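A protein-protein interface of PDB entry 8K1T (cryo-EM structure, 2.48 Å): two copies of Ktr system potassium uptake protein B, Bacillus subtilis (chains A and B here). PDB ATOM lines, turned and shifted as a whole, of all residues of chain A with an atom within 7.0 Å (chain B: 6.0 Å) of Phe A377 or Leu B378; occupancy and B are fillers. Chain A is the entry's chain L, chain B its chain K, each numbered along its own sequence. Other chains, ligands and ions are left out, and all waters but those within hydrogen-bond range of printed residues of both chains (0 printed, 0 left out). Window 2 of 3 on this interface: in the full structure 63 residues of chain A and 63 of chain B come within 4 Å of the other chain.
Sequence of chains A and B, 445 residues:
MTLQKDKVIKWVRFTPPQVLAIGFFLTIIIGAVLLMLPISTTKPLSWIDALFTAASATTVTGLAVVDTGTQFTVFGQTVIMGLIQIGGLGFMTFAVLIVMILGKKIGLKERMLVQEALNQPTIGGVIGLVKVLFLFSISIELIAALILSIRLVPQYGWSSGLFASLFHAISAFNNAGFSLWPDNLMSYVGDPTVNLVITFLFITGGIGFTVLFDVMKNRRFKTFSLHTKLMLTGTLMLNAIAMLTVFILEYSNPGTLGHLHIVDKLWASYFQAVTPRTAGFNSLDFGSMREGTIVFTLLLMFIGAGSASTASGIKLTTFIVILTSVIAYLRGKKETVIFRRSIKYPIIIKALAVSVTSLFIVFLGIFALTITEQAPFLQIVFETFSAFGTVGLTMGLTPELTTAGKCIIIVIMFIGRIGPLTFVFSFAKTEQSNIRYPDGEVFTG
Among the printed residues, merely in contact across the chains: Ala A375 with Glu B291 (3.6 Å), Phe A377 with Glu B291 (3.98 Å), Phe A377 with Val B295 (3.6 Å), Phe A377 with Phe B377 (3.6 Å), Phe A377 with Leu B378 (3.6 Å) and Leu A378 with Phe B377 (3.6 Å).
Printed residues of chain B within 4 Å of Ala A375: Glu B291 (3.6 Å).
Printed residues of chain B within 4 Å of Phe A377: Glu B291, Val B295, Phe B377 and Leu B378.
Printed residues of chain B within 4 Å of Leu A378: Phe B377.
Of the printed residues of chain A, Glu B291 touches Ala A375 and Phe A377.
Of the printed residues of chain A, Val B295 touches Phe A377.
Printed residues of chain A within 4 Å of Phe B377: Phe A377 and Leu A378.
Gln B379 touches none of the printed residues of chain A.
Printed residues of chain A that touch a printed residue of chain B: Ala A375, Phe A377 and Leu A378.
Printed residues of chain B that touch a printed residue of chain A: Glu B291, Val B295, Phe B377 and Leu B378.
Phe A377 touches Glu B291, but with the chains exchanged Glu A291 does not touch Phe B377 (4.04 Å).
Phe A377 touches its own counterpart, Phe B377.
Phe A377 touches Leu B378, and with the chains exchanged Leu A378 touches Phe B377.
Of the 6 pairs that touch across the chains among the printed residues, 3 have their exchanged pair printed and touching as well.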
ATOM      1  N   GLU A 291      11.821   4.679   1.243  1.00  0.00           N
ATOM      2  CA  GLU A 291      11.947   3.343   1.814  1.00  0.00           C
ATOM      3  C   GLU A 291      11.453   2.265   0.860  1.00  0.00           C
ATOM      4  O   GLU A 291      11.937   1.131   0.908  1.00  0.00           O
ATOM      5  CB  GLU A 291      11.192   3.264   3.140  1.00  0.00           C
ATOM      6  CG  GLU A 291      11.793   4.118   4.239  1.00  0.00           C
ATOM      7  CD  GLU A 291      11.023   4.024   5.540  1.00  0.00           C
ATOM      8  OE1 GLU A 291       9.871   3.539   5.519  1.00  0.00           O
ATOM      9  OE2 GLU A 291      11.569   4.434   6.586  1.00  0.00           O
ATOM     10  N   ILE A 366      21.906  -8.978  11.359  1.00  0.00           N
ATOM     11  CA  ILE A 366      20.968  -7.934  11.758  1.00  0.00           C
ATOM     12  C   ILE A 366      20.724  -7.992  13.259  1.00  0.00           C
ATOM     13  O   ILE A 366      20.692  -6.961  13.940  1.00  0.00           O
ATOM     14  CB  ILE A 366      19.656  -8.060  10.965  1.00  0.00           C
ATOM     15  CG1 ILE A 366      19.905  -7.809   9.478  1.00  0.00           C
ATOM     16  CG2 ILE A 366      18.612  -7.100  11.502  1.00  0.00           C
ATOM     17  CD1 ILE A 366      18.687  -7.998   8.614  1.00  0.00           C
ATOM     18  N   PHE A 367      20.549  -9.200  13.797  1.00  0.00           N
ATOM     19  CA  PHE A 367      20.341  -9.353  15.232  1.00  0.00           C
ATOM     20  C   PHE A 367      21.551  -8.871  16.021  1.00  0.00           C
ATOM     21  O   PHE A 367      21.403  -8.191  17.042  1.00  0.00           O
ATOM     22  CB  PHE A 367      20.034 -10.815  15.555  1.00  0.00           C
ATOM     23  CG  PHE A 367      19.797 -11.079  17.011  1.00  0.00           C
ATOM     24  CD1 PHE A 367      18.576 -10.790  17.590  1.00  0.00           C
ATOM     25  CD2 PHE A 367      20.791 -11.628  17.800  1.00  0.00           C
ATOM     26  CE1 PHE A 367      18.354 -11.036  18.927  1.00  0.00           C
ATOM     27  CE2 PHE A 367      20.574 -11.875  19.138  1.00  0.00           C
ATOM     28  CZ  PHE A 367      19.354 -11.578  19.701  1.00  0.00           C
ATOM     29  N   THR A 370      21.973  -4.866  15.831  1.00  0.00           N
ATOM     30  CA  THR A 370      21.030  -4.128  16.666  1.00  0.00           C
ATOM     31  C   THR A 370      21.476  -4.117  18.121  1.00  0.00           C
ATOM     32  O   THR A 370      21.328  -3.107  18.817  1.00  0.00           O
ATOM     33  CB  THR A 370      19.630  -4.724  16.541  1.00  0.00           C
ATOM     34  OG1 THR A 370      19.690  -6.136  16.771  1.00  0.00           O
ATOM     35  CG2 THR A 370      19.062  -4.462  15.161  1.00  0.00           C
ATOM     36  N   ALA A 375      21.520   2.504  15.964  1.00  0.00           N
ATOM     37  CA  ALA A 375      21.322   3.097  14.653  1.00  0.00           C
ATOM     38  C   ALA A 375      19.904   2.797  14.202  1.00  0.00           C
ATOM     39  O   ALA A 375      19.271   1.865  14.710  1.00  0.00           O
ATOM     40  CB  ALA A 375      22.333   2.552  13.635  1.00  0.00           C
ATOM     41  N   PRO A 376      19.367   3.579  13.264  1.00  0.00           N
ATOM     42  CA  PRO A 376      18.038   3.264  12.728  1.00  0.00           C
ATOM     43  C   PRO A 376      18.013   1.878  12.102  1.00  0.00           C
ATOM     44  O   PRO A 376      18.995   1.421  11.517  1.00  0.00           O
ATOM     45  CB  PRO A 376      17.801   4.364  11.686  1.00  0.00           C
ATOM     46  CG  PRO A 376      19.138   4.983  11.448  1.00  0.00           C
ATOM     47  CD  PRO A 376      19.884   4.847  12.728  1.00  0.00           C
ATOM     48  N   PHE A 377      16.869   1.207  12.246  1.00  0.00           N
ATOM     49  CA  PHE A 377      16.774  -0.198  11.866  1.00  0.00           C
ATOM     50  C   PHE A 377      16.964  -0.390  10.366  1.00  0.00           C
ATOM     51  O   PHE A 377      17.563  -1.380   9.935  1.00  0.00           O
ATOM     52  CB  PHE A 377      15.431  -0.763  12.319  1.00  0.00           C
ATOM     53  CG  PHE A 377      15.250  -2.217  12.012  1.00  0.00           C
ATOM     54  CD1 PHE A 377      16.017  -3.171  12.650  1.00  0.00           C
ATOM     55  CD2 PHE A 377      14.302  -2.630  11.097  1.00  0.00           C
ATOM     56  CE1 PHE A 377      15.850  -4.507  12.373  1.00  0.00           C
ATOM     57  CE2 PHE A 377      14.129  -3.966  10.819  1.00  0.00           C
ATOM     58  CZ  PHE A 377      14.902  -4.906  11.458  1.00  0.00           C
ATOM     59  N   LEU A 378      16.453   0.539   9.557  1.00  0.00           N
ATOM     60  CA  LEU A 378      16.570   0.396   8.110  1.00  0.00           C
ATOM     61  C   LEU A 378      18.027   0.419   7.667  1.00  0.00           C
ATOM     62  O   LEU A 378      18.424  -0.342   6.778  1.00  0.00           O
ATOM     63  CB  LEU A 378      15.779   1.496   7.407  1.00  0.00           C
ATOM     64  CG  LEU A 378      15.769   1.429   5.880  1.00  0.00           C
ATOM     65  CD1 LEU A 378      15.216   0.099   5.405  1.00  0.00           C
ATOM     66  CD2 LEU A 378      14.965   2.576   5.307  1.00  0.00           C
ATOM     67  N   GLN A 379      18.838   1.288   8.270  1.00  0.00           N
ATOM     68  CA  GLN A 379      20.254   1.338   7.921  1.00  0.00           C
ATOM     69  C   GLN A 379      20.973   0.061   8.332  1.00  0.00           C
ATOM     70  O   GLN A 379      21.879  -0.400   7.631  1.00  0.00           O
ATOM     71  CB  GLN A 379      20.909   2.557   8.565  1.00  0.00           C
ATOM     72  CG  GLN A 379      20.343   3.875   8.086  1.00  0.00           C
ATOM     73  CD  GLN A 379      21.128   5.062   8.592  1.00  0.00           C
ATOM     74  OE1 GLN A 379      22.156   4.905   9.248  1.00  0.00           O
ATOM     75  NE2 GLN A 379      20.648   6.261   8.288  1.00  0.00           N
ATOM     76  N   ILE A 380      20.593  -0.518   9.472  1.00  0.00           N
ATOM     77  CA  ILE A 380      21.197  -1.774   9.907  1.00  0.00           C
ATOM     78  C   ILE A 380      20.851  -2.898   8.941  1.00  0.00           C
ATOM     79  O   ILE A 380      21.712  -3.703   8.568  1.00  0.00           O
ATOM     80  CB  ILE A 380      20.757  -2.104  11.345  1.00  0.00           C
ATOM     81  CG1 ILE A 380      21.390  -1.125  12.331  1.00  0.00           C
ATOM     82  CG2 ILE A 380      21.109  -3.537  11.700  1.00  0.00           C
ATOM     83  CD1 ILE A 380      21.017  -1.381  13.765  1.00  0.00           C
ATOM     84  N   VAL A 381      19.586  -2.977   8.525  1.00  0.00           N
ATOM     85  CA  VAL A 381      19.174  -4.014   7.584  1.00  0.00           C
ATOM     86  C   VAL A 381      19.857  -3.817   6.238  1.00  0.00           C
ATOM     87  O   VAL A 381      20.331  -4.778   5.622  1.00  0.00           O
ATOM     88  CB  VAL A 381      17.642  -4.028   7.446  1.00  0.00           C
ATOM     89  CG1 VAL A 381      17.209  -5.040   6.405  1.00  0.00           C
ATOM     90  CG2 VAL A 381      17.006  -4.343   8.775  1.00  0.00           C
ATOM     91  N   PHE A 382      19.913  -2.574   5.761  1.00  0.00           N
ATOM     92  CA  PHE A 382      20.555  -2.300   4.482  1.00  0.00           C
ATOM     93  C   PHE A 382      22.039  -2.635   4.528  1.00  0.00           C
ATOM     94  O   PHE A 382      22.592  -3.174   3.564  1.00  0.00           O
ATOM     95  CB  PHE A 382      20.344  -0.838   4.097  1.00  0.00           C
ATOM     96  CG  PHE A 382      20.716  -0.524   2.680  1.00  0.00           C
ATOM     97  CD1 PHE A 382      19.795  -0.676   1.661  1.00  0.00           C
ATOM     98  CD2 PHE A 382      21.982  -0.072   2.366  1.00  0.00           C
ATOM     99  CE1 PHE A 382      20.131  -0.389   0.359  1.00  0.00           C
ATOM    100  CE2 PHE A 382      22.322   0.216   1.063  1.00  0.00           C
ATOM    101  CZ  PHE A 382      21.395   0.058   0.060  1.00  0.00           C
ATOM    102  N   GLU A 383      22.701  -2.316   5.640  1.00  0.00           N
ATOM    103  CA  GLU A 383      24.128  -2.589   5.767  1.00  0.00           C
ATOM    104  C   GLU A 383      24.416  -4.086   5.761  1.00  0.00           C
ATOM    105  O   GLU A 383      25.398  -4.529   5.157  1.00  0.00           O
ATOM    106  CB  GLU A 383      24.665  -1.950   7.046  1.00  0.00           C
ATOM    107  CG  GLU A 383      26.171  -2.002   7.188  1.00  0.00           C
ATOM    108  CD  GLU A 383      26.869  -0.947   6.357  1.00  0.00           C
ATOM    109  OE1 GLU A 383      26.174  -0.109   5.746  1.00  0.00           O
ATOM    110  OE2 GLU A 383      28.116  -0.953   6.319  1.00  0.00           O
ATOM    111  N   GLU B 291      15.530  -3.078  20.066  1.00  0.00           N
ATOM    112  CA  GLU B 291      15.394  -3.632  18.723  1.00  0.00           C
ATOM    113  C   GLU B 291      15.877  -5.072  18.648  1.00  0.00           C
ATOM    114  O   GLU B 291      15.385  -5.846  17.821  1.00  0.00           O
ATOM    115  CB  GLU B 291      16.153  -2.766  17.720  1.00  0.00           C
ATOM    116  CG  GLU B 291      15.562  -1.381  17.534  1.00  0.00           C
ATOM    117  CD  GLU B 291      16.337  -0.544  16.537  1.00  0.00           C
ATOM    118  OE1 GLU B 291      17.483  -0.914  16.209  1.00  0.00           O
ATOM    119  OE2 GLU B 291      15.797   0.486  16.079  1.00  0.00           O
ATOM    120  N   ILE B 294      12.995  -7.204  19.464  1.00  0.00           N
ATOM    121  CA  ILE B 294      12.001  -7.128  18.400  1.00  0.00           C
ATOM    122  C   ILE B 294      12.423  -7.974  17.206  1.00  0.00           C
ATOM    123  O   ILE B 294      11.591  -8.628  16.567  1.00  0.00           O
ATOM    124  CB  ILE B 294      11.764  -5.660  18.008  1.00  0.00           C
ATOM    125  CG1 ILE B 294      11.141  -4.903  19.179  1.00  0.00           C
ATOM    126  CG2 ILE B 294      10.887  -5.565  16.776  1.00  0.00           C
ATOM    127  CD1 ILE B 294      11.080  -3.414  18.975  1.00  0.00           C
ATOM    128  N   VAL B 295      13.718  -7.976  16.883  1.00  0.00           N
ATOM    129  CA  VAL B 295      14.207  -8.781  15.766  1.00  0.00           C
ATOM    130  C   VAL B 295      13.978 -10.261  16.035  1.00  0.00           C
ATOM    131  O   VAL B 295      13.553 -11.010  15.148  1.00  0.00           O
ATOM    132  CB  VAL B 295      15.691  -8.473  15.493  1.00  0.00           C
ATOM    133  CG1 VAL B 295      16.280  -9.492  14.535  1.00  0.00           C
ATOM    134  CG2 VAL B 295      15.840  -7.077  14.927  1.00  0.00           C
ATOM    135  N   LEU B 298      10.358 -11.130  15.567  1.00  0.00           N
ATOM    136  CA  LEU B 298      10.001 -11.266  14.159  1.00  0.00           C
ATOM    137  C   LEU B 298      10.137 -12.709  13.697  1.00  0.00           C
ATOM    138  O   LEU B 298       9.233 -13.260  13.060  1.00  0.00           O
ATOM    139  CB  LEU B 298      10.886 -10.356  13.308  1.00  0.00           C
ATOM    140  CG  LEU B 298      10.353  -9.014  12.821  1.00  0.00           C
ATOM    141  CD1 LEU B 298       9.544  -8.333  13.890  1.00  0.00           C
ATOM    142  CD2 LEU B 298      11.523  -8.143  12.417  1.00  0.00           C
ATOM    143  N   PRO B 376       8.015   4.612  10.737  1.00  0.00           N
ATOM    144  CA  PRO B 376       9.339   4.002  10.895  1.00  0.00           C
ATOM    145  C   PRO B 376       9.352   2.574  10.372  1.00  0.00           C
ATOM    146  O   PRO B 376       8.364   1.845  10.472  1.00  0.00           O
ATOM    147  CB  PRO B 376       9.581   4.057  12.409  1.00  0.00           C
ATOM    148  CG  PRO B 376       8.248   4.341  13.017  1.00  0.00           C
ATOM    149  CD  PRO B 376       7.506   5.147  12.008  1.00  0.00           C
ATOM    150  N   PHE B 377      10.490   2.187   9.795  1.00  0.00           N
ATOM    151  CA  PHE B 377      10.573   0.917   9.082  1.00  0.00           C
ATOM    152  C   PHE B 377      10.378  -0.268  10.018  1.00  0.00           C
ATOM    153  O   PHE B 377       9.769  -1.273   9.635  1.00  0.00           O
ATOM    154  CB  PHE B 377      11.915   0.820   8.359  1.00  0.00           C
ATOM    155  CG  PHE B 377      12.082  -0.434   7.560  1.00  0.00           C
ATOM    156  CD1 PHE B 377      11.309  -0.662   6.439  1.00  0.00           C
ATOM    157  CD2 PHE B 377      13.024  -1.377   7.920  1.00  0.00           C
ATOM    158  CE1 PHE B 377      11.465  -1.811   5.700  1.00  0.00           C
ATOM    159  CE2 PHE B 377      13.186  -2.527   7.183  1.00  0.00           C
ATOM    160  CZ  PHE B 377      12.407  -2.743   6.072  1.00  0.00           C
ATOM    161  N   LEU B 378      10.893  -0.176  11.246  1.00  0.00           N
ATOM    162  CA  LEU B 378      10.769  -1.290  12.179  1.00  0.00           C
ATOM    163  C   LEU B 378       9.311  -1.573  12.516  1.00  0.00           C
ATOM    164  O   LEU B 378       8.905  -2.736  12.619  1.00  0.00           O
ATOM    165  CB  LEU B 378      11.567  -1.003  13.449  1.00  0.00           C
ATOM    166  CG  LEU B 378      11.571  -2.121  14.491  1.00  0.00           C
ATOM    167  CD1 LEU B 378      12.112  -3.408  13.898  1.00  0.00           C
ATOM    168  CD2 LEU B 378      12.382  -1.710  15.701  1.00  0.00           C
ATOM    169  N   GLN B 379       8.509  -0.523  12.696  1.00  0.00           N
ATOM    170  CA  GLN B 379       7.093  -0.720  12.985  1.00  0.00           C
ATOM    171  C   GLN B 379       6.365  -1.339  11.799  1.00  0.00           C
ATOM    172  O   GLN B 379       5.453  -2.152  11.981  1.00  0.00           O
ATOM    173  CB  GLN B 379       6.449   0.604  13.381  1.00  0.00           C
ATOM    174  CG  GLN B 379       7.025   1.205  14.644  1.00  0.00           C
ATOM    175  CD  GLN B 379       6.250   2.414  15.116  1.00  0.00           C
ATOM    176  OE1 GLN B 379       5.223   2.769  14.541  1.00  0.00           O
ATOM    177  NE2 GLN B 379       6.739   3.054  16.170  1.00  0.00           N
ATOM    178  N   ILE B 380       6.744  -0.958  10.579  1.00  0.00           N
ATOM    179  CA  ILE B 380       6.132  -1.545   9.391  1.00  0.00           C
ATOM    180  C   ILE B 380       6.465  -3.027   9.293  1.00  0.00           C
ATOM    181  O   ILE B 380       5.597  -3.855   8.998  1.00  0.00           O
ATOM    182  CB  ILE B 380       6.575  -0.778   8.132  1.00  0.00           C
ATOM    183  CG1 ILE B 380       5.951   0.617   8.116  1.00  0.00           C
ATOM    184  CG2 ILE B 380       6.213  -1.548   6.877  1.00  0.00           C
ATOM    185  CD1 ILE B 380       6.327   1.436   6.911  1.00  0.00           C
ATOM    186  N   VAL B 381       7.728  -3.384   9.530  1.00  0.00           N
ATOM    187  CA  VAL B 381       8.130  -4.786   9.474  1.00  0.00           C
ATOM    188  C   VAL B 381       7.445  -5.583  10.574  1.00  0.00           C
ATOM    189  O   VAL B 381       6.960  -6.696  10.344  1.00  0.00           O
ATOM    190  CB  VAL B 381       9.662  -4.905   9.559  1.00  0.00           C
ATOM    191  CG1 VAL B 381      10.083  -6.361   9.591  1.00  0.00           C
ATOM    192  CG2 VAL B 381      10.299  -4.205   8.387  1.00  0.00           C
ATOM    193  N   PHE B 382       7.395  -5.029  11.787  1.00  0.00           N
ATOM    194  CA  PHE B 382       6.752  -5.724  12.894  1.00  0.00           C
ATOM    195  C   PHE B 382       5.265  -5.919  12.631  1.00  0.00           C
ATOM    196  O   PHE B 382       4.706  -6.975  12.943  1.00  0.00           O
ATOM    197  CB  PHE B 382       6.974  -4.951  14.192  1.00  0.00           C
ATOM    198  CG  PHE B 382       6.599  -5.717  15.425  1.00  0.00           C
ATOM    199  CD1 PHE B 382       7.515  -6.547  16.042  1.00  0.00           C
ATOM    200  CD2 PHE B 382       5.335  -5.605  15.970  1.00  0.00           C
ATOM    201  CE1 PHE B 382       7.178  -7.250  17.175  1.00  0.00           C
ATOM    202  CE2 PHE B 382       4.993  -6.308  17.102  1.00  0.00           C
ATOM    203  CZ  PHE B 382       5.916  -7.131  17.704  1.00  0.00           C
ATOM    204  N   GLU B 383       4.609  -4.907  12.063  1.00  0.00           N
ATOM    205  CA  GLU B 383       3.181  -5.003  11.784  1.00  0.00           C
ATOM    206  C   GLU B 383       2.881  -6.073  10.742  1.00  0.00           C
ATOM    207  O   GLU B 383       1.893  -6.804  10.865  1.00  0.00           O
ATOM    208  CB  GLU B 383       2.653  -3.647  11.320  1.00  0.00           C
ATOM    209  CG  GLU B 383       1.147  -3.573  11.187  1.00  0.00           C
ATOM    210  CD  GLU B 383       0.454  -3.396  12.522  1.00  0.00           C
ATOM    211  OE1 GLU B 383       1.153  -3.231  13.543  1.00  0.00           O
ATOM    212  OE2 GLU B 383      -0.792  -3.417  12.549  1.00  0.00           O
ATOM    213  N   MET B 395       3.588  -2.340  17.667  1.00  0.00           N
ATOM    214  CA  MET B 395       4.496  -1.343  18.204  1.00  0.00           C
ATOM    215  C   MET B 395       3.887   0.050  18.226  1.00  0.00           C
ATOM    216  O   MET B 395       4.568   0.999  18.629  1.00  0.00           O
ATOM    217  CB  MET B 395       5.805  -1.321  17.406  1.00  0.00           C
ATOM    218  CG  MET B 395       6.662  -2.561  17.596  1.00  0.00           C
ATOM    219  SD  MET B 395       8.195  -2.499  16.654  1.00  0.00           S
ATOM    220  CE  MET B 395       8.899  -0.973  17.263  1.00  0.00           C
